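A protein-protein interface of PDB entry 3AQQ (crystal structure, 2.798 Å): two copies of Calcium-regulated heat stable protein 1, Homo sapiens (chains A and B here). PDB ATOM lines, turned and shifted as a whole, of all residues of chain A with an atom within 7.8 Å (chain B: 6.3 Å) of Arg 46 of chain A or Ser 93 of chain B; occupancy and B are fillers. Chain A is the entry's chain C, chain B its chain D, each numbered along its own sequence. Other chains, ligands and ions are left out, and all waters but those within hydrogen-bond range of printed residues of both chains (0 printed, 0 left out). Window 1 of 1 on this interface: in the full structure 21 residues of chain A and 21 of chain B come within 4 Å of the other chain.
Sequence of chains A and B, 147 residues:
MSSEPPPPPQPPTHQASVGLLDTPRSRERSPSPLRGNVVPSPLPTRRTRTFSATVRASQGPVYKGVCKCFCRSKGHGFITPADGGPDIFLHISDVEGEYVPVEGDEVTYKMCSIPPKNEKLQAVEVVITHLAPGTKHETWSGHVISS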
ATOM      1  N   LEU A  43       1.667  16.196 -22.759  1.00  0.00           N
ATOM      2  CA  LEU A  43       0.317  15.644 -22.921  1.00  0.00           C
ATOM      3  C   LEU A  43      -0.612  16.046 -21.764  1.00  0.00           C
ATOM      4  O   LEU A  43      -0.860  15.250 -20.850  1.00  0.00           O
ATOM      5  CB  LEU A  43       0.374  14.115 -23.068  1.00  0.00           C
ATOM      6  CG  LEU A  43      -0.935  13.405 -23.454  1.00  0.00           C
ATOM      7  CD1 LEU A  43      -1.545  12.587 -22.311  1.00  0.00           C
ATOM      8  CD2 LEU A  43      -1.948  14.412 -24.021  1.00  0.00           C
ATOM      9  N   PRO A  44      -1.154  17.275 -21.820  1.00  0.00           N
ATOM     10  CA  PRO A  44      -1.802  17.874 -20.651  1.00  0.00           C
ATOM     11  C   PRO A  44      -3.167  17.273 -20.423  1.00  0.00           C
ATOM     12  O   PRO A  44      -3.893  16.982 -21.370  1.00  0.00           O
ATOM     13  CB  PRO A  44      -1.937  19.351 -21.033  1.00  0.00           C
ATOM     14  CG  PRO A  44      -1.326  19.485 -22.435  1.00  0.00           C
ATOM     15  CD  PRO A  44      -1.319  18.112 -23.016  1.00  0.00           C
ATOM     16  N   THR A  45      -3.506  17.077 -19.161  1.00  0.00           N
ATOM     17  CA  THR A  45      -4.795  16.521 -18.819  1.00  0.00           C
ATOM     18  C   THR A  45      -5.344  17.410 -17.731  1.00  0.00           C
ATOM     19  O   THR A  45      -4.734  18.410 -17.375  1.00  0.00           O
ATOM     20  CB  THR A  45      -4.660  15.097 -18.281  1.00  0.00           C
ATOM     21  OG1 THR A  45      -4.250  15.151 -16.909  1.00  0.00           O
ATOM     22  CG2 THR A  45      -3.639  14.307 -19.096  1.00  0.00           C
ATOM     23  N   ARG A  46      -6.481  17.039 -17.175  1.00  0.00           N
ATOM     24  CA  ARG A  46      -7.147  17.923 -16.243  1.00  0.00           C
ATOM     25  C   ARG A  46      -6.469  18.069 -14.877  1.00  0.00           C
ATOM     26  O   ARG A  46      -6.454  19.157 -14.303  1.00  0.00           O
ATOM     27  CB  ARG A  46      -8.588  17.496 -16.053  1.00  0.00           C
ATOM     28  CG  ARG A  46      -9.412  18.619 -15.498  1.00  0.00           C
ATOM     29  CD  ARG A  46     -10.805  18.147 -15.283  1.00  0.00           C
ATOM     30  NE  ARG A  46     -10.805  16.823 -14.688  1.00  0.00           N
ATOM     31  CZ  ARG A  46     -11.890  16.267 -14.184  1.00  0.00           C
ATOM     32  NH1 ARG A  46     -13.034  16.944 -14.227  1.00  0.00           N
ATOM     33  NH2 ARG A  46     -11.826  15.050 -13.655  1.00  0.00           N
ATOM     34  N   ARG A  47      -5.923  17.002 -14.344  1.00  0.00           N
ATOM     35  CA  ARG A  47      -5.247  17.092 -13.082  1.00  0.00           C
ATOM     36  C   ARG A  47      -3.810  17.271 -13.358  1.00  0.00           C
ATOM     37  O   ARG A  47      -2.994  16.689 -12.719  1.00  0.00           O
ATOM     38  CB  ARG A  47      -5.463  15.824 -12.288  1.00  0.00           C
ATOM     39  CG  ARG A  47      -6.910  15.510 -12.129  1.00  0.00           C
ATOM     40  CD  ARG A  47      -7.179  14.531 -11.062  1.00  0.00           C
ATOM     41  NE  ARG A  47      -8.484  14.771 -10.473  1.00  0.00           N
ATOM     42  CZ  ARG A  47      -9.196  15.862 -10.666  1.00  0.00           C
ATOM     43  NH1 ARG A  47      -8.738  16.814 -11.426  1.00  0.00           N
ATOM     44  NH2 ARG A  47     -10.364  16.003 -10.098  1.00  0.00           N
ATOM     45  N   THR A  48      -3.497  18.069 -14.347  1.00  0.00           N
ATOM     46  CA  THR A  48      -2.132  18.238 -14.744  1.00  0.00           C
ATOM     47  C   THR A  48      -2.060  19.601 -15.332  1.00  0.00           C
ATOM     48  O   THR A  48      -1.034  20.222 -15.353  1.00  0.00           O
ATOM     49  CB  THR A  48      -1.741  17.216 -15.787  1.00  0.00           C
ATOM     50  OG1 THR A  48      -1.052  16.146 -15.160  1.00  0.00           O
ATOM     51  CG2 THR A  48      -0.850  17.813 -16.784  1.00  0.00           C
ATOM     52  N   ARG A  49      -3.181  20.091 -15.797  1.00  0.00           N
ATOM     53  CA  ARG A  49      -3.202  21.425 -16.286  1.00  0.00           C
ATOM     54  C   ARG A  49      -2.777  22.340 -15.178  1.00  0.00           C
ATOM     55  O   ARG A  49      -3.283  22.279 -14.090  1.00  0.00           O
ATOM     56  CB  ARG A  49      -4.588  21.794 -16.753  1.00  0.00           C
ATOM     57  CG  ARG A  49      -4.590  22.837 -17.824  1.00  0.00           C
ATOM     58  CD  ARG A  49      -5.792  22.730 -18.649  1.00  0.00           C
ATOM     59  NE  ARG A  49      -5.669  21.651 -19.594  1.00  0.00           N
ATOM     60  CZ  ARG A  49      -6.527  20.670 -19.684  1.00  0.00           C
ATOM     61  NH1 ARG A  49      -7.551  20.619 -18.896  1.00  0.00           N
ATOM     62  NH2 ARG A  49      -6.346  19.738 -20.557  1.00  0.00           N
ATOM     63  N   THR A  50      -1.852  23.221 -15.481  1.00  0.00           N
ATOM     64  CA  THR A  50      -1.382  24.164 -14.481  1.00  0.00           C
ATOM     65  C   THR A  50      -2.509  25.078 -14.032  1.00  0.00           C
ATOM     66  O   THR A  50      -3.515  25.254 -14.722  1.00  0.00           O
ATOM     67  CB  THR A  50      -0.210  25.039 -14.975  1.00  0.00           C
ATOM     68  OG1 THR A  50      -0.598  25.757 -16.152  1.00  0.00           O
ATOM     69  CG2 THR A  50       0.998  24.197 -15.276  1.00  0.00           C
ATOM     70  N   THR A  54      -5.879  26.578 -16.416  1.00  0.00           N
ATOM     71  CA  THR A  54      -7.249  26.257 -16.053  1.00  0.00           C
ATOM     72  C   THR A  54      -8.071  27.537 -15.935  1.00  0.00           C
ATOM     73  O   THR A  54      -9.098  27.676 -16.590  1.00  0.00           O
ATOM     74  CB  THR A  54      -7.334  25.458 -14.737  1.00  0.00           C
ATOM     75  OG1 THR A  54      -6.383  24.386 -14.751  1.00  0.00           O
ATOM     76  CG2 THR A  54      -8.727  24.889 -14.541  1.00  0.00           C
ATOM     77  N   HIS A  91      -8.264  15.507 -24.806  1.00  0.00           N
ATOM     78  CA  HIS A  91      -7.847  14.436 -23.903  1.00  0.00           C
ATOM     79  C   HIS A  91      -9.046  13.928 -23.128  1.00  0.00           C
ATOM     80  O   HIS A  91      -9.955  14.697 -22.841  1.00  0.00           O
ATOM     81  CB  HIS A  91      -6.756  14.895 -22.931  1.00  0.00           C
ATOM     82  CG  HIS A  91      -6.305  13.807 -22.011  1.00  0.00           C
ATOM     83  ND1 HIS A  91      -7.080  13.351 -20.971  1.00  0.00           N
ATOM     84  CD2 HIS A  91      -5.188  13.044 -22.012  1.00  0.00           C
ATOM     85  CE1 HIS A  91      -6.451  12.364 -20.353  1.00  0.00           C
ATOM     86  NE2 HIS A  91      -5.299  12.163 -20.966  1.00  0.00           N
ATOM     87  N   ILE A  92      -9.052  12.645 -22.778  1.00  0.00           N
ATOM     88  CA  ILE A  92     -10.246  12.032 -22.184  1.00  0.00           C
ATOM     89  C   ILE A  92     -10.693  12.642 -20.860  1.00  0.00           C
ATOM     90  O   ILE A  92     -11.889  12.696 -20.569  1.00  0.00           O
ATOM     91  CB  ILE A  92     -10.111  10.505 -22.010  1.00  0.00           C
ATOM     92  CG1 ILE A  92     -11.268   9.959 -21.170  1.00  0.00           C
ATOM     93  CG2 ILE A  92      -8.779  10.151 -21.386  1.00  0.00           C
ATOM     94  CD1 ILE A  92     -11.281   8.456 -21.062  1.00  0.00           C
ATOM     95  N   SER A  93      -9.740  13.108 -20.063  1.00  0.00           N
ATOM     96  CA  SER A  93     -10.047  13.648 -18.735  1.00  0.00           C
ATOM     97  C   SER A  93     -10.865  14.939 -18.775  1.00  0.00           C
ATOM     98  O   SER A  93     -11.361  15.394 -17.750  1.00  0.00           O
ATOM     99  CB  SER A  93      -8.759  13.905 -17.957  1.00  0.00           C
ATOM    100  OG  SER A  93      -7.998  14.937 -18.567  1.00  0.00           O
ATOM    101  N   ASP A  94     -10.988  15.534 -19.957  1.00  0.00           N
ATOM    102  CA  ASP A  94     -11.624  16.832 -20.078  1.00  0.00           C
ATOM    103  C   ASP A  94     -13.079  16.741 -20.500  1.00  0.00           C
ATOM    104  O   ASP A  94     -13.794  17.746 -20.564  1.00  0.00           O
ATOM    105  CB  ASP A  94     -10.820  17.691 -21.032  1.00  0.00           C
ATOM    106  CG  ASP A  94      -9.523  18.165 -20.409  1.00  0.00           C
ATOM    107  OD1 ASP A  94      -9.614  18.797 -19.336  1.00  0.00           O
ATOM    108  OD2 ASP A  94      -8.428  17.909 -20.975  1.00  0.00           O
ATOM    109  N   VAL A  95     -13.507  15.511 -20.776  1.00  0.00           N
ATOM    110  CA  VAL A  95     -14.865  15.234 -21.229  1.00  0.00           C
ATOM    111  C   VAL A  95     -15.815  15.117 -20.037  1.00  0.00           C
ATOM    112  O   VAL A  95     -15.567  14.359 -19.099  1.00  0.00           O
ATOM    113  CB  VAL A  95     -14.902  13.959 -22.109  1.00  0.00           C
ATOM    114  N   GLU A  96     -16.899  15.881 -20.084  1.00  0.00           N
ATOM    115  CA  GLU A  96     -17.899  15.870 -19.029  1.00  0.00           C
ATOM    116  C   GLU A  96     -19.162  15.111 -19.468  1.00  0.00           C
ATOM    117  O   GLU A  96     -19.792  15.488 -20.444  1.00  0.00           O
ATOM    118  CB  GLU A  96     -18.232  17.311 -18.628  1.00  0.00           C
ATOM    119  N   GLN A 122      -5.655  22.967 -26.772  1.00  0.00           N
ATOM    120  CA  GLN A 122      -6.409  21.873 -26.214  1.00  0.00           C
ATOM    121  C   GLN A 122      -7.813  22.299 -25.911  1.00  0.00           C
ATOM    122  O   GLN A 122      -8.049  23.420 -25.557  1.00  0.00           O
ATOM    123  CB  GLN A 122      -5.757  21.395 -24.941  1.00  0.00           C
ATOM    124  CG  GLN A 122      -6.361  20.165 -24.410  1.00  0.00           C
ATOM    125  CD  GLN A 122      -5.466  19.457 -23.477  1.00  0.00           C
ATOM    126  OE1 GLN A 122      -4.445  19.972 -23.082  1.00  0.00           O
ATOM    127  NE2 GLN A 122      -5.845  18.266 -23.104  1.00  0.00           N
ATOM    128  N   VAL A 124     -11.118  21.990 -23.498  1.00  0.00           N
ATOM    129  CA  VAL A 124     -11.404  21.717 -22.084  1.00  0.00           C
ATOM    130  C   VAL A 124     -12.873  21.977 -21.738  1.00  0.00           C
ATOM    131  O   VAL A 124     -13.559  22.704 -22.449  1.00  0.00           O
ATOM    132  CB  VAL A 124     -10.491  22.571 -21.132  1.00  0.00           C
ATOM    133  CG1 VAL A 124      -9.020  22.297 -21.385  1.00  0.00           C
ATOM    134  CG2 VAL A 124     -10.792  24.065 -21.265  1.00  0.00           C
ATOM    135  N   GLU A 125     -13.337  21.400 -20.631  1.00  0.00           N
ATOM    136  CA  GLU A 125     -14.714  21.596 -20.189  1.00  0.00           C
ATOM    137  C   GLU A 125     -15.633  21.257 -21.361  1.00  0.00           C
ATOM    138  O   GLU A 125     -16.388  22.097 -21.844  1.00  0.00           O
ATOM    139  CB  GLU A 125     -14.933  23.043 -19.699  1.00  0.00           C
ATOM    140  CG  GLU A 125     -14.589  23.271 -18.224  1.00  0.00           C
ATOM    141  CD  GLU A 125     -14.138  24.711 -17.889  1.00  0.00           C
ATOM    142  OE1 GLU A 125     -14.979  25.644 -17.903  1.00  0.00           O
ATOM    143  OE2 GLU A 125     -12.931  24.910 -17.590  1.00  0.00           O
ATOM    144  N   PRO B  44     -23.707  11.553  -7.703  1.00  0.00           N
ATOM    145  CA  PRO B  44     -23.434  11.540  -9.150  1.00  0.00           C
ATOM    146  C   PRO B  44     -22.103  12.173  -9.514  1.00  0.00           C
ATOM    147  O   PRO B  44     -21.714  13.192  -8.940  1.00  0.00           O
ATOM    148  CB  PRO B  44     -24.580  12.381  -9.743  1.00  0.00           C
ATOM    149  CG  PRO B  44     -25.517  12.662  -8.594  1.00  0.00           C
ATOM    150  CD  PRO B  44     -24.666  12.618  -7.372  1.00  0.00           C
ATOM    151  N   THR B  45     -21.416  11.568 -10.474  1.00  0.00           N
ATOM    152  CA  THR B  45     -20.105  12.048 -10.852  1.00  0.00           C
ATOM    153  C   THR B  45     -20.127  12.573 -12.266  1.00  0.00           C
ATOM    154  O   THR B  45     -21.165  12.592 -12.915  1.00  0.00           O
ATOM    155  CB  THR B  45     -19.037  10.939 -10.753  1.00  0.00           C
ATOM    156  OG1 THR B  45     -19.436   9.821 -11.559  1.00  0.00           O
ATOM    157  CG2 THR B  45     -18.844  10.489  -9.296  1.00  0.00           C
ATOM    158  N   ARG B  46     -18.963  13.002 -12.730  1.00  0.00           N
ATOM    159  CA  ARG B  46     -18.824  13.625 -14.032  1.00  0.00           C
ATOM    160  C   ARG B  46     -18.885  12.590 -15.149  1.00  0.00           C
ATOM    161  O   ARG B  46     -19.012  12.945 -16.310  1.00  0.00           O
ATOM    162  CB  ARG B  46     -17.501  14.375 -14.089  1.00  0.00           C
ATOM    163  CG  ARG B  46     -17.399  15.369 -15.230  1.00  0.00           C
ATOM    164  CD  ARG B  46     -15.948  15.751 -15.436  1.00  0.00           C
ATOM    165  NE  ARG B  46     -15.106  14.590 -15.215  1.00  0.00           N
ATOM    166  CZ  ARG B  46     -13.961  14.374 -15.851  1.00  0.00           C
ATOM    167  NH1 ARG B  46     -13.524  15.250 -16.747  1.00  0.00           N
ATOM    168  NH2 ARG B  46     -13.256  13.276 -15.606  1.00  0.00           N
ATOM    169  N   ARG B  47     -18.775  11.317 -14.782  1.00  0.00           N
ATOM    170  CA  ARG B  47     -18.822  10.214 -15.728  1.00  0.00           C
ATOM    171  C   ARG B  47     -20.181   9.559 -15.599  1.00  0.00           C
ATOM    172  O   ARG B  47     -20.612   8.779 -16.450  1.00  0.00           O
ATOM    173  CB  ARG B  47     -17.753   9.187 -15.387  1.00  0.00           C
ATOM    174  CG  ARG B  47     -16.363   9.708 -15.483  1.00  0.00           C
ATOM    175  CD  ARG B  47     -15.756   9.381 -16.827  1.00  0.00           C
ATOM    176  NE  ARG B  47     -15.157  10.562 -17.441  1.00  0.00           N
ATOM    177  CZ  ARG B  47     -14.068  10.531 -18.204  1.00  0.00           C
ATOM    178  NH1 ARG B  47     -13.441   9.374 -18.429  1.00  0.00           N
ATOM    179  NH2 ARG B  47     -13.601  11.660 -18.726  1.00  0.00           N
ATOM    180  N   ARG B  49     -22.941  11.553 -14.612  1.00  0.00           N
ATOM    181  CA  ARG B  49     -23.924  12.593 -14.908  1.00  0.00           C
ATOM    182  C   ARG B  49     -24.695  12.343 -16.220  1.00  0.00           C
ATOM    183  O   ARG B  49     -24.107  12.243 -17.308  1.00  0.00           O
ATOM    184  CB  ARG B  49     -23.256  13.981 -14.905  1.00  0.00           C
ATOM    185  CG  ARG B  49     -24.229  15.169 -14.854  1.00  0.00           C
ATOM    186  CD  ARG B  49     -23.569  16.454 -14.314  1.00  0.00           C
ATOM    187  NE  ARG B  49     -23.040  16.316 -12.945  1.00  0.00           N
ATOM    188  CZ  ARG B  49     -21.745  16.319 -12.631  1.00  0.00           C
ATOM    189  NH1 ARG B  49     -20.838  16.463 -13.579  1.00  0.00           N
ATOM    190  NH2 ARG B  49     -21.351  16.182 -11.372  1.00  0.00           N
ATOM    191  N   GLY B  75     -12.935  12.034  -1.409  1.00  0.00           N
ATOM    192  CA  GLY B  75     -13.332  12.466  -2.740  1.00  0.00           C
ATOM    193  C   GLY B  75     -14.456  13.491  -2.837  1.00  0.00           C
ATOM    194  O   GLY B  75     -15.171  13.543  -3.846  1.00  0.00           O
ATOM    195  N   HIS B  91     -18.115  16.982  -5.821  1.00  0.00           N
ATOM    196  CA  HIS B  91     -17.422  15.714  -5.970  1.00  0.00           C
ATOM    197  C   HIS B  91     -16.062  15.950  -6.586  1.00  0.00           C
ATOM    198  O   HIS B  91     -15.875  16.898  -7.347  1.00  0.00           O
ATOM    199  CB  HIS B  91     -18.222  14.719  -6.810  1.00  0.00           C
ATOM    200  CG  HIS B  91     -17.572  13.381  -6.906  1.00  0.00           C
ATOM    201  ND1 HIS B  91     -16.532  13.117  -7.772  1.00  0.00           N
ATOM    202  CD2 HIS B  91     -17.761  12.239  -6.201  1.00  0.00           C
ATOM    203  CE1 HIS B  91     -16.132  11.872  -7.616  1.00  0.00           C
ATOM    204  NE2 HIS B  91     -16.864  11.314  -6.666  1.00  0.00           N
ATOM    205  N   ILE B  92     -15.106  15.096  -6.248  1.00  0.00           N
ATOM    206  CA  ILE B  92     -13.756  15.263  -6.762  1.00  0.00           C
ATOM    207  C   ILE B  92     -13.689  15.328  -8.290  1.00  0.00           C
ATOM    208  O   ILE B  92     -13.012  16.194  -8.837  1.00  0.00           O
ATOM    209  CB  ILE B  92     -12.781  14.194  -6.233  1.00  0.00           C
ATOM    210  CG1 ILE B  92     -11.357  14.498  -6.703  1.00  0.00           C
ATOM    211  CG2 ILE B  92     -13.217  12.813  -6.649  1.00  0.00           C
ATOM    212  CD1 ILE B  92     -10.308  13.555  -6.142  1.00  0.00           C
ATOM    213  N   SER B  93     -14.392  14.429  -8.970  1.00  0.00           N
ATOM    214  CA  SER B  93     -14.376  14.335 -10.440  1.00  0.00           C
ATOM    215  C   SER B  93     -14.589  15.663 -11.157  1.00  0.00           C
ATOM    216  O   SER B  93     -14.077  15.864 -12.245  1.00  0.00           O
ATOM    217  CB  SER B  93     -15.453  13.354 -10.897  1.00  0.00           C
ATOM    218  OG  SER B  93     -16.743  13.820 -10.521  1.00  0.00           O
ATOM    219  N   ASP B  94     -15.343  16.561 -10.532  1.00  0.00           N
ATOM    220  CA  ASP B  94     -15.733  17.821 -11.149  1.00  0.00           C
ATOM    221  C   ASP B  94     -14.715  18.951 -11.000  1.00  0.00           C
ATOM    222  O   ASP B  94     -14.925  20.056 -11.495  1.00  0.00           O
ATOM    223  CB  ASP B  94     -17.070  18.250 -10.569  1.00  0.00           C
ATOM    224  CG  ASP B  94     -18.201  17.410 -11.085  1.00  0.00           C
ATOM    225  OD1 ASP B  94     -18.302  17.297 -12.326  1.00  0.00           O
ATOM    226  OD2 ASP B  94     -18.978  16.866 -10.269  1.00  0.00           O
ATOM    227  N   VAL B  95     -13.617  18.663 -10.306  1.00  0.00           N
ATOM    228  CA  VAL B  95     -12.540  19.619 -10.083  1.00  0.00           C
ATOM    229  C   VAL B  95     -11.559  19.629 -11.247  1.00  0.00           C
ATOM    230  O   VAL B  95     -10.992  18.603 -11.598  1.00  0.00           O
ATOM    231  CB  VAL B  95     -11.751  19.272  -8.788  1.00  0.00           C
ATOM    232  CG1 VAL B  95     -10.449  20.064  -8.704  1.00  0.00           C
ATOM    233  CG2 VAL B  95     -12.608  19.502  -7.574  1.00  0.00           C
ATOM    234  N   GLU B  96     -11.335  20.795 -11.833  1.00  0.00           N
ATOM    235  CA  GLU B  96     -10.270  20.912 -12.813  1.00  0.00           C
ATOM    236  C   GLU B  96      -9.058  21.686 -12.322  1.00  0.00           C
ATOM    237  O   GLU B  96      -9.178  22.613 -11.524  1.00  0.00           O
ATOM    238  CB  GLU B  96     -10.788  21.518 -14.099  1.00  0.00           C
ATOM    239  CG  GLU B  96     -11.874  22.524 -13.914  1.00  0.00           C
ATOM    240  CD  GLU B  96     -12.790  22.498 -15.101  1.00  0.00           C
ATOM    241  OE1 GLU B  96     -13.250  23.571 -15.546  1.00  0.00           O
ATOM    242  OE2 GLU B  96     -13.041  21.376 -15.596  1.00  0.00           O
ATOM    243  N   GLY B  97      -7.891  21.286 -12.813  1.00  0.00           N
ATOM    244  CA  GLY B  97      -6.631  21.897 -12.446  1.00  0.00           C
ATOM    245  C   GLY B  97      -5.796  20.896 -11.680  1.00  0.00           C
ATOM    246  O   GLY B  97      -6.313  19.845 -11.270  1.00  0.00           O
ATOM    247  N   GLU B  98      -4.520  21.239 -11.475  1.00  0.00           N
ATOM    248  CA  GLU B  98      -3.545  20.409 -10.741  1.00  0.00           C
ATOM    249  C   GLU B  98      -3.696  20.390  -9.225  1.00  0.00           C
ATOM    250  O   GLU B  98      -3.169  19.495  -8.573  1.00  0.00           O
ATOM    251  CB  GLU B  98      -2.130  20.888 -11.038  1.00  0.00           C
ATOM    252  CG  GLU B  98      -1.931  22.346 -10.684  1.00  0.00           C
ATOM    253  CD  GLU B  98      -0.597  22.897 -11.149  1.00  0.00           C
ATOM    254  OE1 GLU B  98       0.383  22.122 -11.166  1.00  0.00           O
ATOM    255  OE2 GLU B  98      -0.534  24.104 -11.491  1.00  0.00           O
ATOM    256  N   GLN B 122     -25.489  20.759  -6.686  1.00  0.00           N
ATOM    257  CA  GLN B 122     -24.139  20.260  -6.853  1.00  0.00           C
ATOM    258  C   GLN B 122     -23.349  21.257  -7.661  1.00  0.00           C
ATOM    259  O   GLN B 122     -23.919  22.122  -8.312  1.00  0.00           O
ATOM    260  CB  GLN B 122     -24.160  18.907  -7.541  1.00  0.00           C
ATOM    261  CG  GLN B 122     -22.814  18.214  -7.652  1.00  0.00           C
ATOM    262  CD  GLN B 122     -22.958  16.814  -8.248  1.00  0.00           C
ATOM    263  OE1 GLN B 122     -24.059  16.384  -8.590  1.00  0.00           O
ATOM    264  NE2 GLN B 122     -21.847  16.101  -8.369  1.00  0.00           N
ATOM    265  N   TRP B 140      -2.503  16.727  -7.028  1.00  0.00           N
ATOM    266  CA  TRP B 140      -2.798  15.301  -7.101  1.00  0.00           C
ATOM    267  C   TRP B 140      -1.478  14.579  -7.356  1.00  0.00           C
ATOM    268  O   TRP B 140      -0.646  15.074  -8.115  1.00  0.00           O
ATOM    269  CB  TRP B 140      -3.829  15.019  -8.208  1.00  0.00           C
ATOM    270  CG  TRP B 140      -4.887  16.106  -8.326  1.00  0.00           C
ATOM    271  CD1 TRP B 140      -4.858  17.194  -9.159  1.00  0.00           C
ATOM    272  CD2 TRP B 140      -6.098  16.219  -7.565  1.00  0.00           C
ATOM    273  NE1 TRP B 140      -5.975  17.970  -8.966  1.00  0.00           N
ATOM    274  CE2 TRP B 140      -6.752  17.398  -7.992  1.00  0.00           C
ATOM    275  CE3 TRP B 140      -6.693  15.445  -6.566  1.00  0.00           C
ATOM    276  CZ2 TRP B 140      -7.968  17.817  -7.453  1.00  0.00           C
ATOM    277  CZ3 TRP B 140      -7.903  15.860  -6.038  1.00  0.00           C
ATOM    278  CH2 TRP B 140      -8.526  17.036  -6.483  1.00  0.00           C
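The backbone carbonyl oxygen (O) of Ser 93 of chain B is in hydrogen-bond range of the guanidinium group (NH1) of Arg 46 of chain A, at 2.5 Å.
N of Gly 97 of chain B is in hydrogen-bond range of O of Arg 46 of chain A, 3.0 Å away.
NH2 of Arg 47 of chain A is in hydrogen-bond range of O of Ile 92 of chain B (2.9 Å).
The guanidinium group (NH1) of Arg 47 of chain A lies within hydrogen-bond range of the backbone carbonyl oxygen (O) of Val 95 of chain B (2.9 Å).
The backbone carbonyl oxygen (O) of Arg 49 of chain A sits at hydrogen-bond distance from the backbone NH (N) of Glu 98 of chain B, at 3.1 Å.
The backbone carbonyl oxygen (O) of Ile 92 of chain A sits at hydrogen-bond distance from the guanidinium group (NH2) of Arg 47 of chain B.
The backbone carbonyl oxygen (O) of Val 95 of chain A is in hydrogen-bond range of the guanidinium group (NH1) of Arg 46 of chain B (3.2 Å).
The backbone carbonyl oxygen (O) of Val 95 of chain A lies within hydrogen-bond range of the guanidinium group (NH2) of Arg 47 of chain B (3.4 Å).
The side-chain carboxylate of Glu 125 of chain A lies close to the side-chain carboxylate of Glu 96 of chain B.
NH2 of Arg 46 of chain A sits close to NH2 of Arg 46 of chain B (3.0 Å).
The backbone carbonyl oxygen (O) of Ser 93 of chain A sits close to the guanidinium group (NH1) of Arg 46 of chain B (2.4 Å).
NE2 of Gln 122 of chain A sits close to NH2 of Arg 49 of chain A, at 3.0 Å.
OG1 of Thr 54 of chain A sits at hydrogen-bond distance from O of Thr 50 of chain A (3.0 Å).
ND1 of His 91 of chain A lies within hydrogen-bond range of N of Ser 93 of chain A (2.8 Å).
OG of Ser 93 of chain B sits at hydrogen-bond distance from N of Arg 46 of chain B (3.2 Å).
NE1 of Trp 140 of chain B sits at hydrogen-bond distance from O of Gly 97 of chain B (3.0 Å).
The backbone carbonyl oxygen (O) of Glu 98 of chain B sits close to the indole nitrogen (NE1) of Trp 140 of chain B (3.2 Å).
Among the printed residues, pairs that only touch across the chains: Arg 46 of chain A with Val 95 of chain B, Arg 46 of chain A with Glu 96 of chain B, Arg 47 of chain A with Gly 97 of chain B, Arg 47 of chain A with Trp 140 of chain B, Arg 49 of chain A with Gly 97 of chain B, Thr 50 of chain A with Glu 98 of chain B, Thr 54 of chain A with Glu 96 of chain B, Thr 54 of chain A with Gly 97 of chain B and Glu 96 of chain A with Arg 46 of chain B.
Gly 97 of chain B touches just these residues of chain A: Arg 46, Arg 47, Arg 49 and Thr 54.
Of the printed residues of chain A, Trp 140 of chain B touches Arg 47.
Of the printed residues of chain B, Val 95 of chain A touches Arg 46 and Arg 47.
Gln 122 of chain B touches none of the printed residues of chain A.
Leu 43 of chain A touches none of the printed residues of chain B.
The nearest printed residue of chain B that does not touch Arg 46 of chain A is Glu 98 of chain B (4.01 Å).
Of the 16 printed residues of chain B, 9 touch a printed residue of chain A.
Of the 18 printed residues of chain A, 10 touch a printed residue of chain B.
Printed residues of chain A that touch a printed residue of chain B: Arg 46, Arg 47, Arg 49, Thr 50, Thr 54, Ile 92, Ser 93, Val 95, Glu 96 and Glu 125.
Among the printed residues, 20 pairs touch across the chains.
Among the printed residues, no Asp or Glu carboxylate lies within 4 Å of a Lys or Arg side-chain nitrogen of the other chain.
Arg 46 of chain A touches Ser 93 of chain B, and with the chains exchanged Ser 93 of chain A touches Arg 46 of chain B.
Arg 46 of chain A touches Val 95 of chain B, and with the chains exchanged Val 95 of chain A touches Arg 46 of chain B.
Arg 46 of chain A touches Glu 96 of chain B, and with the chains exchanged Glu 96 of chain A touches Arg 46 of chain B.
Arg 47 of chain A touches Val 95 of chain B, and with the chains exchanged Val 95 of chain A touches Arg 47 of chain B.
Positions printed for both chains: 44, 45, 46, 47, 49, 91, 92, 93, 94, 95, 96 and 122.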
